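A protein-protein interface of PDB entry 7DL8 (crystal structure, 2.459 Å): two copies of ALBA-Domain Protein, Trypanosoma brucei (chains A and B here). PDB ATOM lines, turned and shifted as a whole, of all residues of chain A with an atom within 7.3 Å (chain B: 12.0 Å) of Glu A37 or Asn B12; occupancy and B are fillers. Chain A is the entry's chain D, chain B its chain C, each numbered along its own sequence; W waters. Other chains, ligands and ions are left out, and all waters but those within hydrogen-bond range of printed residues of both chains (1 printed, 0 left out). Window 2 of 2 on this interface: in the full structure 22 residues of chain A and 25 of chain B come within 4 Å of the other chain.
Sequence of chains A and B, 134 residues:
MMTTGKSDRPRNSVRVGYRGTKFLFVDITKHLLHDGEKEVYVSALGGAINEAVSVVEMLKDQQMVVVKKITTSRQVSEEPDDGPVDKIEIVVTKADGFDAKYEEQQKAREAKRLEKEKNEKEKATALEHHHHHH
His A31 touches none of the printed residues of chain B. No residue of chain B comes within 4 Å of Leu A33. No residue of chain B comes within 4 Å of Gly A36. Of chain B, only Arg B11 (3.6 Å) and Asn B12 (3.2 Å) come within 4 Å of Glu A37. No residue of chain B comes within 4 Å of Lys A38. Of chain B, only Asn B12 (3.5 Å) comes within 4 Å of Glu A39. Printed residues of chain B within 4 Å of Tyr A41: Asn B12, Ser B13 and Val B14. Of the printed residues of chain B, Val A42 touches Val B14 and Val B16. Of the printed residues of chain A, Arg B11 touches Leu A32 (3.4 Å) and Glu A37 (3.6 Å). Of chain A, only Glu A37 (3.2 Å), Glu A39 (3.5 Å), Val A40 (3.4 Å) and Tyr A41 (2.9 Å) come within 4 Å of Asn B12. Of the printed residues of chain A, Val B14 touches Leu A32, Val A40, Tyr A41 and Val A42. Arg B15 touches none of the printed residues of chain A. Printed residues of chain A within 4 Å of Val B16: Val A42 (3.9 Å). The nearest printed residue of chain B that does not touch Glu A37 is Ser B13 (6.5 Å). The nearest residue of chain A that does not touch Asn B12 is Leu A32 (4.7 Å). The nearest printed residue of chain A that does not touch Val B16 is Thr A29 (6.6 Å).
Among the printed residues, merely in contact across the chains: Leu A32 with Arg B11 (3.4 Å), Leu A32 with Val B14 (3.6 Å), Glu A37 with Arg B11 (3.6 Å), Glu A37 with Asn B12 (3.2 Å), Glu A39 with Asn B12 (3.5 Å), Val A40 with Asn B12 (3.4 Å), Val A40 with Val B14 (3.7 Å), Tyr A41 with Ser B13 (3.5 Å), Val A42 with Val B14 (3.5 Å) and Val A42 with Val B16 (3.9 Å).
No position is printed for both chains. Of the 12 pairs that touch across the chains among the printed residues, none has its exchanged pair printed and touching as well.
N of Tyr A41 is in hydrogen-bond range of O of Asn B12, at 2.9 Å. N of Val B14 sits at hydrogen-bond distance from O of Tyr A41, at 2.8 Å.
Water W1 bridges the side-chain hydroxyl (OG) of Ser B13 and the backbone carbonyl oxygen (O) of Tyr A41.
The backbone NH of Glu A37 lies close to the backbone carbonyl oxygen of Leu A32. The side-chain carboxylate (OE2) of Glu A39 sits at hydrogen-bond distance from the side-chain hydroxyl (OH) of Tyr A41 (3.4 Å). N of Val A40 sits at hydrogen-bond distance from O of Val A92 (2.9 Å).
Of the 16 printed residues of chain A, 6 touch a printed residue of chain B. Hydrophobic or aromatic side chains of chain A within 4 Å of the printed part of chain B: Leu A32, Val A40, Tyr A41 and Val A42. Along chain A the printed residues that touch a printed residue of chain B span positions 32 to 42. Of the 7 printed residues of chain B, 5 touch a printed residue of chain A. Among the printed residues, 12 pairs touch across the chains. Among the printed residues, no Asp or Glu carboxylate lies within 4 Å of a Lys or Arg side-chain nitrogen of the other chain.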
ATOM      1  N   THR A  29     -12.133  26.031  22.356  1.00  0.00           N
ATOM      2  CA  THR A  29     -12.962  26.985  21.625  1.00  0.00           C
ATOM      3  C   THR A  29     -13.046  26.625  20.146  1.00  0.00           C
ATOM      4  O   THR A  29     -14.119  26.713  19.539  1.00  0.00           O
ATOM      5  CB  THR A  29     -12.416  28.403  21.802  1.00  0.00           C
ATOM      6  OG1 THR A  29     -12.194  28.662  23.193  1.00  0.00           O
ATOM      7  CG2 THR A  29     -13.401  29.425  21.254  1.00  0.00           C
ATOM      8  N   HIS A  31     -12.715  23.609  18.837  1.00  0.00           N
ATOM      9  CA  HIS A  31     -13.512  22.395  18.695  1.00  0.00           C
ATOM     10  C   HIS A  31     -15.001  22.685  18.843  1.00  0.00           C
ATOM     11  O   HIS A  31     -15.823  22.117  18.113  1.00  0.00           O
ATOM     12  CB  HIS A  31     -13.070  21.353  19.722  1.00  0.00           C
ATOM     13  CG  HIS A  31     -11.947  20.482  19.252  1.00  0.00           C
ATOM     14  ND1 HIS A  31     -12.149  19.216  18.747  1.00  0.00           N
ATOM     15  CD2 HIS A  31     -10.611  20.694  19.214  1.00  0.00           C
ATOM     16  CE1 HIS A  31     -10.984  18.686  18.415  1.00  0.00           C
ATOM     17  NE2 HIS A  31     -10.036  19.562  18.690  1.00  0.00           N
ATOM     18  N   LEU A  32     -15.368  23.568  19.776  1.00  0.00           N
ATOM     19  CA  LEU A  32     -16.782  23.858  19.995  1.00  0.00           C
ATOM     20  C   LEU A  32     -17.389  24.602  18.813  1.00  0.00           C
ATOM     21  O   LEU A  32     -18.535  24.337  18.432  1.00  0.00           O
ATOM     22  CB  LEU A  32     -16.960  24.656  21.286  1.00  0.00           C
ATOM     23  CG  LEU A  32     -16.853  23.834  22.571  1.00  0.00           C
ATOM     24  CD1 LEU A  32     -16.864  24.734  23.791  1.00  0.00           C
ATOM     25  CD2 LEU A  32     -17.976  22.814  22.643  1.00  0.00           C
ATOM     26  N   LEU A  33     -16.635  25.521  18.207  1.00  0.00           N
ATOM     27  CA  LEU A  33     -17.143  26.214  17.028  1.00  0.00           C
ATOM     28  C   LEU A  33     -17.281  25.254  15.854  1.00  0.00           C
ATOM     29  O   LEU A  33     -18.244  25.338  15.084  1.00  0.00           O
ATOM     30  CB  LEU A  33     -16.228  27.383  16.667  1.00  0.00           C
ATOM     31  CG  LEU A  33     -16.280  28.592  17.601  1.00  0.00           C
ATOM     32  CD1 LEU A  33     -15.332  29.677  17.122  1.00  0.00           C
ATOM     33  CD2 LEU A  33     -17.700  29.125  17.707  1.00  0.00           C
ATOM     34  N   HIS A  34     -16.331  24.329  15.710  1.00  0.00           N
ATOM     35  CA  HIS A  34     -16.408  23.341  14.640  1.00  0.00           C
ATOM     36  C   HIS A  34     -17.523  22.333  14.889  1.00  0.00           C
ATOM     37  O   HIS A  34     -18.095  21.796  13.933  1.00  0.00           O
ATOM     38  CB  HIS A  34     -15.063  22.631  14.490  1.00  0.00           C
ATOM     39  CG  HIS A  34     -15.135  21.360  13.698  1.00  0.00           C
ATOM     40  ND1 HIS A  34     -15.205  21.345  12.325  1.00  0.00           N
ATOM     41  CD2 HIS A  34     -15.146  20.066  14.096  1.00  0.00           C
ATOM     42  CE1 HIS A  34     -15.257  20.089  11.905  1.00  0.00           C
ATOM     43  NE2 HIS A  34     -15.223  19.298  12.958  1.00  0.00           N
ATOM     44  N   ASP A  35     -17.854  22.074  16.153  1.00  0.00           N
ATOM     45  CA  ASP A  35     -18.858  21.071  16.513  1.00  0.00           C
ATOM     46  C   ASP A  35     -20.245  21.667  16.711  1.00  0.00           C
ATOM     47  O   ASP A  35     -20.963  21.287  17.641  1.00  0.00           O
ATOM     48  CB  ASP A  35     -18.409  20.325  17.766  1.00  0.00           C
ATOM     49  CG  ASP A  35     -18.491  18.820  17.610  1.00  0.00           C
ATOM     50  OD1 ASP A  35     -18.588  18.343  16.459  1.00  0.00           O
ATOM     51  OD2 ASP A  35     -18.457  18.112  18.639  1.00  0.00           O
ATOM     52  N   GLY A  36     -20.652  22.605  15.853  1.00  0.00           N
ATOM     53  CA  GLY A  36     -22.017  23.067  15.772  1.00  0.00           C
ATOM     54  C   GLY A  36     -22.279  24.428  16.391  1.00  0.00           C
ATOM     55  O   GLY A  36     -23.177  25.141  15.928  1.00  0.00           O
ATOM     56  N   GLU A  37     -21.529  24.804  17.424  1.00  0.00           N
ATOM     57  CA  GLU A  37     -21.806  26.056  18.119  1.00  0.00           C
ATOM     58  C   GLU A  37     -21.526  27.244  17.207  1.00  0.00           C
ATOM     59  O   GLU A  37     -20.450  27.344  16.609  1.00  0.00           O
ATOM     60  CB  GLU A  37     -20.966  26.159  19.393  1.00  0.00           C
ATOM     61  CG  GLU A  37     -21.051  24.945  20.310  1.00  0.00           C
ATOM     62  CD  GLU A  37     -22.387  24.827  21.023  1.00  0.00           C
ATOM     63  OE1 GLU A  37     -23.211  25.760  20.917  1.00  0.00           O
ATOM     64  OE2 GLU A  37     -22.609  23.798  21.695  1.00  0.00           O
ATOM     65  N   LYS A  38     -22.500  28.151  17.107  1.00  0.00           N
ATOM     66  CA  LYS A  38     -22.319  29.359  16.311  1.00  0.00           C
ATOM     67  C   LYS A  38     -21.459  30.385  17.036  1.00  0.00           C
ATOM     68  O   LYS A  38     -20.737  31.153  16.389  1.00  0.00           O
ATOM     69  CB  LYS A  38     -23.677  29.966  15.952  1.00  0.00           C
ATOM     70  N   GLU A  39     -21.525  30.411  18.364  1.00  0.00           N
ATOM     71  CA  GLU A  39     -20.769  31.356  19.171  1.00  0.00           C
ATOM     72  C   GLU A  39     -20.349  30.669  20.462  1.00  0.00           C
ATOM     73  O   GLU A  39     -21.073  29.827  21.000  1.00  0.00           O
ATOM     74  CB  GLU A  39     -21.589  32.619  19.477  1.00  0.00           C
ATOM     75  CG  GLU A  39     -22.870  32.351  20.253  1.00  0.00           C
ATOM     76  CD  GLU A  39     -23.870  33.485  20.151  1.00  0.00           C
ATOM     77  OE1 GLU A  39     -23.542  34.519  19.532  1.00  0.00           O
ATOM     78  OE2 GLU A  39     -24.987  33.343  20.692  1.00  0.00           O
ATOM     79  N   VAL A  40     -19.166  31.032  20.948  1.00  0.00           N
ATOM     80  CA  VAL A  40     -18.617  30.499  22.190  1.00  0.00           C
ATOM     81  C   VAL A  40     -18.377  31.663  23.142  1.00  0.00           C
ATOM     82  O   VAL A  40     -17.826  32.695  22.744  1.00  0.00           O
ATOM     83  CB  VAL A  40     -17.322  29.707  21.939  1.00  0.00           C
ATOM     84  CG1 VAL A  40     -16.543  29.519  23.233  1.00  0.00           C
ATOM     85  CG2 VAL A  40     -17.642  28.360  21.309  1.00  0.00           C
ATOM     86  N   TYR A  41     -18.791  31.492  24.397  1.00  0.00           N
ATOM     87  CA  TYR A  41     -18.628  32.507  25.430  1.00  0.00           C
ATOM     88  C   TYR A  41     -17.368  32.186  26.227  1.00  0.00           C
ATOM     89  O   TYR A  41     -17.352  31.240  27.021  1.00  0.00           O
ATOM     90  CB  TYR A  41     -19.851  32.556  26.344  1.00  0.00           C
ATOM     91  CG  TYR A  41     -21.107  33.085  25.684  1.00  0.00           C
ATOM     92  CD1 TYR A  41     -21.772  32.344  24.715  1.00  0.00           C
ATOM     93  CD2 TYR A  41     -21.635  34.320  26.039  1.00  0.00           C
ATOM     94  CE1 TYR A  41     -22.919  32.821  24.112  1.00  0.00           C
ATOM     95  CE2 TYR A  41     -22.784  34.804  25.442  1.00  0.00           C
ATOM     96  CZ  TYR A  41     -23.420  34.050  24.479  1.00  0.00           C
ATOM     97  OH  TYR A  41     -24.564  34.527  23.880  1.00  0.00           O
ATOM     98  N   VAL A  42     -16.318  32.972  26.016  1.00  0.00           N
ATOM     99  CA  VAL A  42     -15.051  32.798  26.714  1.00  0.00           C
ATOM    100  C   VAL A  42     -15.050  33.750  27.902  1.00  0.00           C
ATOM    101  O   VAL A  42     -15.072  34.974  27.730  1.00  0.00           O
ATOM    102  CB  VAL A  42     -13.854  33.053  25.788  1.00  0.00           C
ATOM    103  CG1 VAL A  42     -12.547  32.865  26.546  1.00  0.00           C
ATOM    104  CG2 VAL A  42     -13.911  32.131  24.580  1.00  0.00           C
ATOM    105  N   VAL A  92     -17.153  34.957  20.827  1.00  0.00           N
ATOM    106  CA  VAL A  92     -16.450  34.788  19.566  1.00  0.00           C
ATOM    107  C   VAL A  92     -17.295  33.909  18.657  1.00  0.00           C
ATOM    108  O   VAL A  92     -17.990  32.994  19.110  1.00  0.00           O
ATOM    109  CB  VAL A  92     -15.036  34.190  19.758  1.00  0.00           C
ATOM    110  CG1 VAL A  92     -14.216  35.059  20.698  1.00  0.00           C
ATOM    111  CG2 VAL A  92     -15.114  32.763  20.278  1.00  0.00           C
ATOM    112  N   THR A  93     -17.243  34.208  17.366  1.00  0.00           N
ATOM    113  CA  THR A  93     -17.894  33.412  16.340  1.00  0.00           C
ATOM    114  C   THR A  93     -16.851  32.992  15.315  1.00  0.00           C
ATOM    115  O   THR A  93     -15.705  33.446  15.342  1.00  0.00           O
ATOM    116  CB  THR A  93     -19.031  34.187  15.659  1.00  0.00           C
ATOM    117  OG1 THR A  93     -18.481  35.210  14.819  1.00  0.00           O
ATOM    118  CG2 THR A  93     -19.946  34.825  16.693  1.00  0.00           C
ATOM    119  N   LYS A  94     -17.261  32.115  14.405  1.00  0.00           N
ATOM    120  CA  LYS A  94     -16.347  31.645  13.376  1.00  0.00           C
ATOM    121  C   LYS A  94     -15.908  32.803  12.492  1.00  0.00           C
ATOM    122  O   LYS A  94     -16.706  33.674  12.137  1.00  0.00           O
ATOM    123  CB  LYS A  94     -17.023  30.582  12.511  1.00  0.00           C
ATOM    124  CG  LYS A  94     -16.873  29.153  12.987  1.00  0.00           C
ATOM    125  CD  LYS A  94     -17.758  28.242  12.149  1.00  0.00           C
ATOM    126  CE  LYS A  94     -17.446  26.777  12.379  1.00  0.00           C
ATOM    127  NZ  LYS A  94     -18.235  25.896  11.473  1.00  0.00           N
ATOM    128  N   PRO B  10     -23.409  24.640  30.424  1.00  0.00           N
ATOM    129  CA  PRO B  10     -23.568  25.305  29.127  1.00  0.00           C
ATOM    130  C   PRO B  10     -22.498  24.865  28.133  1.00  0.00           C
ATOM    131  O   PRO B  10     -21.322  25.172  28.323  1.00  0.00           O
ATOM    132  CB  PRO B  10     -23.424  26.794  29.466  1.00  0.00           C
ATOM    133  CG  PRO B  10     -23.602  26.883  30.952  1.00  0.00           C
ATOM    134  CD  PRO B  10     -23.088  25.594  31.498  1.00  0.00           C
ATOM    135  N   ARG B  11     -22.915  24.157  27.079  1.00  0.00           N
ATOM    136  CA  ARG B  11     -21.954  23.547  26.167  1.00  0.00           C
ATOM    137  C   ARG B  11     -21.115  24.598  25.449  1.00  0.00           C
ATOM    138  O   ARG B  11     -19.916  24.394  25.222  1.00  0.00           O
ATOM    139  CB  ARG B  11     -22.686  22.664  25.155  1.00  0.00           C
ATOM    140  N   ASN B  12     -21.722  25.731  25.085  1.00  0.00           N
ATOM    141  CA  ASN B  12     -21.029  26.780  24.343  1.00  0.00           C
ATOM    142  C   ASN B  12     -20.386  27.829  25.246  1.00  0.00           C
ATOM    143  O   ASN B  12     -20.205  28.977  24.816  1.00  0.00           O
ATOM    144  CB  ASN B  12     -21.992  27.451  23.362  1.00  0.00           C
ATOM    145  CG  ASN B  12     -23.128  28.175  24.061  1.00  0.00           C
ATOM    146  OD1 ASN B  12     -23.369  27.975  25.253  1.00  0.00           O
ATOM    147  ND2 ASN B  12     -23.828  29.027  23.322  1.00  0.00           N
ATOM    148  N   SER B  13     -20.019  27.470  26.473  1.00  0.00           N
ATOM    149  CA  SER B  13     -19.385  28.390  27.408  1.00  0.00           C
ATOM    150  C   SER B  13     -18.062  27.792  27.855  1.00  0.00           C
ATOM    151  O   SER B  13     -18.039  26.708  28.450  1.00  0.00           O
ATOM    152  CB  SER B  13     -20.295  28.662  28.609  1.00  0.00           C
ATOM    153  OG  SER B  13     -19.553  28.978  29.773  1.00  0.00           O
ATOM    154  N   VAL B  14     -16.968  28.491  27.575  1.00  0.00           N
ATOM    155  CA  VAL B  14     -15.633  28.046  27.958  1.00  0.00           C
ATOM    156  C   VAL B  14     -15.168  28.915  29.112  1.00  0.00           C
ATOM    157  O   VAL B  14     -15.013  30.133  28.956  1.00  0.00           O
ATOM    158  CB  VAL B  14     -14.637  28.109  26.788  1.00  0.00           C
ATOM    159  CG1 VAL B  14     -13.246  27.725  27.268  1.00  0.00           C
ATOM    160  CG2 VAL B  14     -15.077  27.188  25.670  1.00  0.00           C
ATOM    161  N   ARG B  15     -14.935  28.295  30.267  1.00  0.00           N
ATOM    162  CA  ARG B  15     -14.478  28.997  31.458  1.00  0.00           C
ATOM    163  C   ARG B  15     -12.973  28.797  31.574  1.00  0.00           C
ATOM    164  O   ARG B  15     -12.504  27.683  31.832  1.00  0.00           O
ATOM    165  CB  ARG B  15     -15.201  28.492  32.705  1.00  0.00           C
ATOM    166  CG  ARG B  15     -14.516  28.868  34.016  1.00  0.00           C
ATOM    167  CD  ARG B  15     -14.566  30.369  34.250  1.00  0.00           C
ATOM    168  NE  ARG B  15     -15.696  30.751  35.092  1.00  0.00           N
ATOM    169  CZ  ARG B  15     -16.756  31.421  34.654  1.00  0.00           C
ATOM    170  NH1 ARG B  15     -17.744  31.729  35.484  1.00  0.00           N
ATOM    171  NH2 ARG B  15     -16.832  31.776  33.380  1.00  0.00           N
ATOM    172  N   VAL B  16     -12.221  29.873  31.385  1.00  0.00           N
ATOM    173  CA  VAL B  16     -10.769  29.811  31.469  1.00  0.00           C
ATOM    174  C   VAL B  16     -10.360  29.885  32.933  1.00  0.00           C
ATOM    175  O   VAL B  16     -10.783  30.791  33.662  1.00  0.00           O
ATOM    176  CB  VAL B  16     -10.130  30.948  30.655  1.00  0.00           C
ATOM    177  CG1 VAL B  16      -8.618  30.945  30.828  1.00  0.00           C
ATOM    178  CG2 VAL B  16     -10.507  30.831  29.186  1.00  0.00           C
HETATM  179  O   HOH W   1     -18.818  31.384  29.668  1.00  0.00           O
